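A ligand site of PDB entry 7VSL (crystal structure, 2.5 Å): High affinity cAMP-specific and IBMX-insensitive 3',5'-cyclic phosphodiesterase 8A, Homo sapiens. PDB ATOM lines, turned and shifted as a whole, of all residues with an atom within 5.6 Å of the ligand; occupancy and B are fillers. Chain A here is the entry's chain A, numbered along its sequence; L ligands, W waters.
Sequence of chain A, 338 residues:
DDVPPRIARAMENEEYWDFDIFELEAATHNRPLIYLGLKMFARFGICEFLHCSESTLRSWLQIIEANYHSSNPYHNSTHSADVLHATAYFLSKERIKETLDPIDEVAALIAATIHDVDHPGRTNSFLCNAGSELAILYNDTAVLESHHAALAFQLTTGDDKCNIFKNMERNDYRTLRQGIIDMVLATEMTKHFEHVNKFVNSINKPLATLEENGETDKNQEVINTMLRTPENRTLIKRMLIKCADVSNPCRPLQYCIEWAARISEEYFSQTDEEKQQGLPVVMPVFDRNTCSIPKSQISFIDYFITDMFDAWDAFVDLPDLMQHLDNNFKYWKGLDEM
The side-chain amide nitrogen of Asn 248 sits at hydrogen-bond distance from a nitrogen (N4) of the ligand (2.9 Å).
N5 of the ligand is in hydrogen-bond range of OE1 of Gln 297 (3.1 Å).
The side-chain amide nitrogen of Asn 248 lies within hydrogen-bond range of the side-chain hydroxyl of Tyr 74, at 3.3 Å.
The side-chain amino group (NZ) of Lys 242 is in hydrogen-bond range of a ring nitrogen (ND1) of His 192 (3.2 Å).
O of Thr 187 lies close to F2 of the ligand, 2.9 Å away.
ND1 of His 192 sits close to F1 of the ligand.
Tyr 74 touches the ligand (OH to C1, 3.3 Å).
Glu 188 touches the ligand (C to F2, 3.9 Å).
CA of Met 189 touches F2 of the ligand, 3.3 Å away.
NZ of Lys 242 touches F1 of the ligand (3.7 Å).
Val 246 touches the ligand (CG1 to C13, 3.6 Å).
Ile 263 touches the ligand.
OH of Tyr 267 touches C8 of the ligand, at 3.3 Å.
CZ of Phe 286 touches CL1 of the ligand, at 3.4 Å.
CE2 of Phe 300 touches C3 of the ligand, at 3.3 Å.
CE2 of Phe 304 touches C10 of the ligand, at 3.7 Å.
Of the 20 residues printed, 14 come within 4 Å of the ligand.
Along chain A the residues within 4 Å of the ligand span positions 74 to 304.
Water W1 lies within hydrogen-bond range of OD2 of Asp 245 (2.8 Å) and O of Thr 187 (3.1 Å).
Water W2 lies within hydrogen-bond range of the side-chain hydroxyl (OH) of Tyr 74 (2.9 Å) and the backbone carbonyl oxygen (O) of Asp 245 (3.3 Å).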
ATOM      1  N   TYR A  74      19.515  13.227  24.705  1.00  0.00           N
ATOM      2  CA  TYR A  74      20.621  14.175  24.806  1.00  0.00           C
ATOM      3  C   TYR A  74      20.247  15.559  24.280  1.00  0.00           C
ATOM      4  O   TYR A  74      20.403  16.574  24.979  1.00  0.00           O
ATOM      5  CB  TYR A  74      21.837  13.612  24.062  1.00  0.00           C
ATOM      6  CG  TYR A  74      23.101  14.431  24.133  1.00  0.00           C
ATOM      7  CD1 TYR A  74      24.084  14.161  25.089  1.00  0.00           C
ATOM      8  CD2 TYR A  74      23.338  15.455  23.221  1.00  0.00           C
ATOM      9  CE1 TYR A  74      25.254  14.904  25.137  1.00  0.00           C
ATOM     10  CE2 TYR A  74      24.488  16.191  23.260  1.00  0.00           C
ATOM     11  CZ  TYR A  74      25.450  15.922  24.208  1.00  0.00           C
ATOM     12  OH  TYR A  74      26.582  16.669  24.179  1.00  0.00           O
ATOM     13  N   HIS A  75      19.737  15.625  23.052  1.00  0.00           N
ATOM     14  CA  HIS A  75      19.612  16.897  22.326  1.00  0.00           C
ATOM     15  C   HIS A  75      18.316  17.613  22.717  1.00  0.00           C
ATOM     16  O   HIS A  75      17.410  17.857  21.911  1.00  0.00           O
ATOM     17  CB  HIS A  75      19.727  16.633  20.828  1.00  0.00           C
ATOM     18  CG  HIS A  75      21.144  16.589  20.355  1.00  0.00           C
ATOM     19  ND1 HIS A  75      21.679  15.501  19.719  1.00  0.00           N
ATOM     20  CD2 HIS A  75      22.153  17.481  20.497  1.00  0.00           C
ATOM     21  CE1 HIS A  75      22.958  15.717  19.460  1.00  0.00           C
ATOM     22  NE2 HIS A  75      23.269  16.921  19.929  1.00  0.00           N
ATOM     23  N   THR A 187      29.606  24.225  14.493  1.00  0.00           N
ATOM     24  CA  THR A 187      29.424  23.011  15.264  1.00  0.00           C
ATOM     25  C   THR A 187      29.269  21.772  14.394  1.00  0.00           C
ATOM     26  O   THR A 187      29.302  20.674  14.937  1.00  0.00           O
ATOM     27  CB  THR A 187      28.218  23.159  16.181  1.00  0.00           C
ATOM     28  OG1 THR A 187      27.005  23.359  15.422  1.00  0.00           O
ATOM     29  CG2 THR A 187      28.419  24.337  17.106  1.00  0.00           C
ATOM     30  N   GLU A 188      29.131  21.929  13.069  1.00  0.00           N
ATOM     31  CA  GLU A 188      28.972  20.787  12.165  1.00  0.00           C
ATOM     32  C   GLU A 188      30.189  19.873  12.228  1.00  0.00           C
ATOM     33  O   GLU A 188      31.340  20.318  12.186  1.00  0.00           O
ATOM     34  CB  GLU A 188      28.759  21.260  10.719  1.00  0.00           C
ATOM     35  CG  GLU A 188      28.453  20.090   9.755  1.00  0.00           C
ATOM     36  CD  GLU A 188      28.380  20.531   8.308  1.00  0.00           C
ATOM     37  OE1 GLU A 188      29.002  21.556   7.945  1.00  0.00           O
ATOM     38  OE2 GLU A 188      27.699  19.846   7.511  1.00  0.00           O
ATOM     39  N   MET A 189      29.908  18.577  12.302  1.00  0.00           N
ATOM     40  CA  MET A 189      30.960  17.601  12.506  1.00  0.00           C
ATOM     41  C   MET A 189      31.981  17.614  11.383  1.00  0.00           C
ATOM     42  O   MET A 189      33.188  17.539  11.643  1.00  0.00           O
ATOM     43  CB  MET A 189      30.357  16.205  12.660  1.00  0.00           C
ATOM     44  CG  MET A 189      31.374  15.171  13.092  1.00  0.00           C
ATOM     45  SD  MET A 189      30.669  13.551  12.964  1.00  0.00           S
ATOM     46  CE  MET A 189      30.855  13.261  11.198  1.00  0.00           C
ATOM     47  N   HIS A 192      35.203  19.549  11.620  1.00  0.00           N
ATOM     48  CA  HIS A 192      35.852  19.488  12.925  1.00  0.00           C
ATOM     49  C   HIS A 192      37.350  19.754  12.824  1.00  0.00           C
ATOM     50  O   HIS A 192      37.858  20.708  13.431  1.00  0.00           O
ATOM     51  CB  HIS A 192      35.616  18.133  13.576  1.00  0.00           C
ATOM     52  CG  HIS A 192      36.485  17.916  14.768  1.00  0.00           C
ATOM     53  ND1 HIS A 192      36.255  18.526  15.971  1.00  0.00           N
ATOM     54  CD2 HIS A 192      37.629  17.213  14.907  1.00  0.00           C
ATOM     55  CE1 HIS A 192      37.207  18.192  16.827  1.00  0.00           C
ATOM     56  NE2 HIS A 192      38.055  17.391  16.206  1.00  0.00           N
ATOM     57  N   LYS A 242      32.751  25.199  19.780  1.00  0.00           N
ATOM     58  CA  LYS A 242      33.024  23.802  19.499  1.00  0.00           C
ATOM     59  C   LYS A 242      33.421  23.050  20.775  1.00  0.00           C
ATOM     60  O   LYS A 242      33.032  21.898  20.967  1.00  0.00           O
ATOM     61  CB  LYS A 242      34.134  23.669  18.443  1.00  0.00           C
ATOM     62  CG  LYS A 242      33.673  23.788  17.014  1.00  0.00           C
ATOM     63  CD  LYS A 242      34.887  23.664  16.081  1.00  0.00           C
ATOM     64  CE  LYS A 242      35.562  22.306  16.241  1.00  0.00           C
ATOM     65  NZ  LYS A 242      34.588  21.208  16.232  1.00  0.00           N
ATOM     66  N   ASP A 245      30.268  22.938  23.171  1.00  0.00           N
ATOM     67  CA  ASP A 245      29.328  21.953  22.668  1.00  0.00           C
ATOM     68  C   ASP A 245      29.666  20.538  23.142  1.00  0.00           C
ATOM     69  O   ASP A 245      28.753  19.770  23.510  1.00  0.00           O
ATOM     70  CB  ASP A 245      29.268  22.011  21.143  1.00  0.00           C
ATOM     71  CG  ASP A 245      28.201  21.111  20.577  1.00  0.00           C
ATOM     72  OD1 ASP A 245      27.224  20.835  21.282  1.00  0.00           O
ATOM     73  OD2 ASP A 245      28.335  20.676  19.425  1.00  0.00           O
ATOM     74  N   VAL A 246      30.954  20.143  23.133  1.00  0.00           N
ATOM     75  CA  VAL A 246      31.334  18.780  23.530  1.00  0.00           C
ATOM     76  C   VAL A 246      32.256  18.860  24.757  1.00  0.00           C
ATOM     77  O   VAL A 246      33.330  18.246  24.806  1.00  0.00           O
ATOM     78  CB  VAL A 246      31.992  18.013  22.374  1.00  0.00           C
ATOM     79  CG1 VAL A 246      30.994  17.810  21.277  1.00  0.00           C
ATOM     80  CG2 VAL A 246      33.148  18.764  21.843  1.00  0.00           C
ATOM     81  N   ASN A 248      31.272  17.802  27.727  1.00  0.00           N
ATOM     82  CA  ASN A 248      30.863  16.817  28.727  1.00  0.00           C
ATOM     83  C   ASN A 248      31.980  15.854  29.150  1.00  0.00           C
ATOM     84  O   ASN A 248      32.033  15.527  30.343  1.00  0.00           O
ATOM     85  CB  ASN A 248      29.578  16.072  28.283  1.00  0.00           C
ATOM     86  CG  ASN A 248      29.682  15.333  26.950  1.00  0.00           C
ATOM     87  OD1 ASN A 248      30.032  14.139  26.899  1.00  0.00           O
ATOM     88  ND2 ASN A 248      29.298  16.012  25.864  1.00  0.00           N
ATOM     89  N   PRO A 249      32.932  15.435  28.297  1.00  0.00           N
ATOM     90  CA  PRO A 249      34.028  14.569  28.811  1.00  0.00           C
ATOM     91  C   PRO A 249      34.971  15.278  29.797  1.00  0.00           C
ATOM     92  O   PRO A 249      35.706  14.597  30.506  1.00  0.00           O
ATOM     93  CB  PRO A 249      34.771  14.135  27.530  1.00  0.00           C
ATOM     94  CG  PRO A 249      33.748  14.219  26.485  1.00  0.00           C
ATOM     95  CD  PRO A 249      32.948  15.464  26.820  1.00  0.00           C
ATOM     96  N   TRP A 259      25.950  12.179  30.582  1.00  0.00           N
ATOM     97  CA  TRP A 259      26.006  12.648  29.196  1.00  0.00           C
ATOM     98  C   TRP A 259      26.324  11.507  28.239  1.00  0.00           C
ATOM     99  O   TRP A 259      25.712  11.394  27.176  1.00  0.00           O
ATOM    100  CB  TRP A 259      27.004  13.801  29.059  1.00  0.00           C
ATOM    101  CG  TRP A 259      26.538  15.101  29.692  1.00  0.00           C
ATOM    102  CD1 TRP A 259      27.160  15.804  30.683  1.00  0.00           C
ATOM    103  CD2 TRP A 259      25.325  15.831  29.393  1.00  0.00           C
ATOM    104  NE1 TRP A 259      26.428  16.909  30.996  1.00  0.00           N
ATOM    105  CE2 TRP A 259      25.295  16.949  30.221  1.00  0.00           C
ATOM    106  CE3 TRP A 259      24.261  15.625  28.507  1.00  0.00           C
ATOM    107  CZ2 TRP A 259      24.233  17.874  30.194  1.00  0.00           C
ATOM    108  CZ3 TRP A 259      23.209  16.550  28.478  1.00  0.00           C
ATOM    109  CH2 TRP A 259      23.209  17.656  29.311  1.00  0.00           C
ATOM    110  N   ALA A 260      27.274  10.626  28.614  1.00  0.00           N
ATOM    111  CA  ALA A 260      27.557   9.441  27.796  1.00  0.00           C
ATOM    112  C   ALA A 260      26.310   8.572  27.602  1.00  0.00           C
ATOM    113  O   ALA A 260      26.036   8.106  26.491  1.00  0.00           O
ATOM    114  CB  ALA A 260      28.676   8.605  28.425  1.00  0.00           C
ATOM    115  N   ILE A 263      23.716  10.515  25.145  1.00  0.00           N
ATOM    116  CA  ILE A 263      24.041  10.498  23.727  1.00  0.00           C
ATOM    117  C   ILE A 263      24.054   9.068  23.184  1.00  0.00           C
ATOM    118  O   ILE A 263      23.664   8.825  22.032  1.00  0.00           O
ATOM    119  CB  ILE A 263      25.380  11.228  23.478  1.00  0.00           C
ATOM    120  CG1 ILE A 263      25.553  11.421  21.971  1.00  0.00           C
ATOM    121  CG2 ILE A 263      26.542  10.509  24.133  1.00  0.00           C
ATOM    122  CD1 ILE A 263      24.513  12.344  21.420  1.00  0.00           C
ATOM    123  N   TYR A 267      21.810   7.619  20.000  1.00  0.00           N
ATOM    124  CA  TYR A 267      22.334   6.928  18.822  1.00  0.00           C
ATOM    125  C   TYR A 267      21.821   5.496  18.704  1.00  0.00           C
ATOM    126  O   TYR A 267      21.747   4.968  17.580  1.00  0.00           O
ATOM    127  CB  TYR A 267      23.863   6.925  18.813  1.00  0.00           C
ATOM    128  CG  TYR A 267      24.471   8.288  18.612  1.00  0.00           C
ATOM    129  CD1 TYR A 267      25.808   8.541  18.965  1.00  0.00           C
ATOM    130  CD2 TYR A 267      23.715   9.335  18.081  1.00  0.00           C
ATOM    131  CE1 TYR A 267      26.368   9.820  18.786  1.00  0.00           C
ATOM    132  CE2 TYR A 267      24.265  10.614  17.903  1.00  0.00           C
ATOM    133  CZ  TYR A 267      25.582  10.847  18.255  1.00  0.00           C
ATOM    134  OH  TYR A 267      26.059  12.131  18.055  1.00  0.00           O
ATOM    135  N   PHE A 286      27.161   1.781  17.240  1.00  0.00           N
ATOM    136  CA  PHE A 286      26.247   2.293  18.258  1.00  0.00           C
ATOM    137  C   PHE A 286      24.897   1.595  18.136  1.00  0.00           C
ATOM    138  O   PHE A 286      23.867   2.164  17.758  1.00  0.00           O
ATOM    139  CB  PHE A 286      26.132   3.802  18.164  1.00  0.00           C
ATOM    140  CG  PHE A 286      27.122   4.541  19.027  1.00  0.00           C
ATOM    141  CD1 PHE A 286      26.838   4.806  20.360  1.00  0.00           C
ATOM    142  CD2 PHE A 286      28.362   4.954  18.510  1.00  0.00           C
ATOM    143  CE1 PHE A 286      27.762   5.475  21.168  1.00  0.00           C
ATOM    144  CE2 PHE A 286      29.275   5.613  19.317  1.00  0.00           C
ATOM    145  CZ  PHE A 286      28.980   5.869  20.640  1.00  0.00           C
ATOM    146  N   SER A 296      33.372   2.939  23.593  1.00  0.00           N
ATOM    147  CA  SER A 296      33.007   3.936  22.601  1.00  0.00           C
ATOM    148  C   SER A 296      33.351   5.348  23.092  1.00  0.00           C
ATOM    149  O   SER A 296      33.743   6.198  22.296  1.00  0.00           O
ATOM    150  CB  SER A 296      31.529   3.838  22.250  1.00  0.00           C
ATOM    151  OG  SER A 296      31.252   2.552  21.723  1.00  0.00           O
ATOM    152  N   GLN A 297      33.225   5.603  24.406  1.00  0.00           N
ATOM    153  CA  GLN A 297      33.604   6.905  24.945  1.00  0.00           C
ATOM    154  C   GLN A 297      35.095   7.140  24.788  1.00  0.00           C
ATOM    155  O   GLN A 297      35.519   8.254  24.462  1.00  0.00           O
ATOM    156  CB  GLN A 297      33.194   7.008  26.407  1.00  0.00           C
ATOM    157  CG  GLN A 297      31.710   7.048  26.550  1.00  0.00           C
ATOM    158  CD  GLN A 297      31.148   8.290  25.868  1.00  0.00           C
ATOM    159  OE1 GLN A 297      31.774   9.338  25.907  1.00  0.00           O
ATOM    160  NE2 GLN A 297      29.991   8.164  25.231  1.00  0.00           N
ATOM    161  N   PHE A 300      35.651   8.002  21.229  1.00  0.00           N
ATOM    162  CA  PHE A 300      35.184   9.361  21.036  1.00  0.00           C
ATOM    163  C   PHE A 300      36.212  10.367  21.523  1.00  0.00           C
ATOM    164  O   PHE A 300      36.580  11.298  20.784  1.00  0.00           O
ATOM    165  CB  PHE A 300      33.853   9.538  21.736  1.00  0.00           C
ATOM    166  CG  PHE A 300      33.315  10.913  21.635  1.00  0.00           C
ATOM    167  CD1 PHE A 300      32.806  11.391  20.427  1.00  0.00           C
ATOM    168  CD2 PHE A 300      33.326  11.760  22.740  1.00  0.00           C
ATOM    169  CE1 PHE A 300      32.319  12.665  20.324  1.00  0.00           C
ATOM    170  CE2 PHE A 300      32.839  13.042  22.648  1.00  0.00           C
ATOM    171  CZ  PHE A 300      32.329  13.502  21.426  1.00  0.00           C
ATOM    172  N   PHE A 304      37.932  13.068  18.783  1.00  0.00           N
ATOM    173  CA  PHE A 304      37.461  14.451  18.748  1.00  0.00           C
ATOM    174  C   PHE A 304      37.953  15.308  19.922  1.00  0.00           C
ATOM    175  O   PHE A 304      38.201  16.501  19.743  1.00  0.00           O
ATOM    176  CB  PHE A 304      35.929  14.491  18.722  1.00  0.00           C
ATOM    177  CG  PHE A 304      35.294  13.833  17.527  1.00  0.00           C
ATOM    178  CD1 PHE A 304      35.245  14.470  16.294  1.00  0.00           C
ATOM    179  CD2 PHE A 304      34.686  12.585  17.645  1.00  0.00           C
ATOM    180  CE1 PHE A 304      34.638  13.859  15.175  1.00  0.00           C
ATOM    181  CE2 PHE A 304      34.072  11.971  16.546  1.00  0.00           C
ATOM    182  CZ  PHE A 304      34.043  12.608  15.312  1.00  0.00           C
HETATM  183  N1  LIG L   1      30.041  10.749  23.036  1.00  0.00           N
HETATM  184  C1  LIG L   1      28.631  14.869  22.393  1.00  0.00           C
HETATM  185  C2  LIG L   1      29.364  12.988  23.059  1.00  0.00           C
HETATM  186  C3  LIG L   1      29.895  11.890  23.739  1.00  0.00           C
HETATM  187  N2  LIG L   1      29.141  11.704  21.035  1.00  0.00           N
HETATM  188  C4  LIG L   1      29.016  12.843  21.746  1.00  0.00           C
HETATM  189  C5  LIG L   1      29.648  10.738  21.772  1.00  0.00           C
HETATM  190  N3  LIG L   1      28.532  14.041  21.312  1.00  0.00           N
HETATM  191  N4  LIG L   1      29.116  14.321  23.480  1.00  0.00           N
HETATM  192  N5  LIG L   1      30.230  11.878  25.027  1.00  0.00           N
HETATM  193 CL1  LIG L   1      29.736   9.185  20.994  1.00  0.00          CL
HETATM  194  C6  LIG L   1      28.021  14.376  19.988  1.00  0.00           C
HETATM  195  C7  LIG L   1      29.089  14.286  18.924  1.00  0.00           C
HETATM  196  C8  LIG L   1      29.253  13.118  18.204  1.00  0.00           C
HETATM  197  C9  LIG L   1      30.243  13.011  17.247  1.00  0.00           C
HETATM  198  C10 LIG L   1      31.088  14.064  16.997  1.00  0.00           C
HETATM  199  C11 LIG L   1      30.912  15.246  17.700  1.00  0.00           C
HETATM  200  C12 LIG L   1      29.933  15.361  18.667  1.00  0.00           C
HETATM  201  O1  LIG L   1      31.802  16.185  17.221  1.00  0.00           O
HETATM  202  C13 LIG L   1      31.821  17.511  17.774  1.00  0.00           C
HETATM  203  C14 LIG L   1      31.973  18.414  16.453  1.00  0.00           C
HETATM  204  F1  LIG L   1      32.951  17.905  15.653  1.00  0.00           F
HETATM  205  F2  LIG L   1      30.834  18.356  15.713  1.00  0.00           F
HETATM  206  O   HOH W   1      30.575  20.910  17.775  1.00  0.00           O
HETATM  207  O   HOH W   2      27.290  17.636  21.530  1.00  0.00           O
HETATM  208  O   HOH W   3      33.026  20.703  18.812  1.00  0.00           O
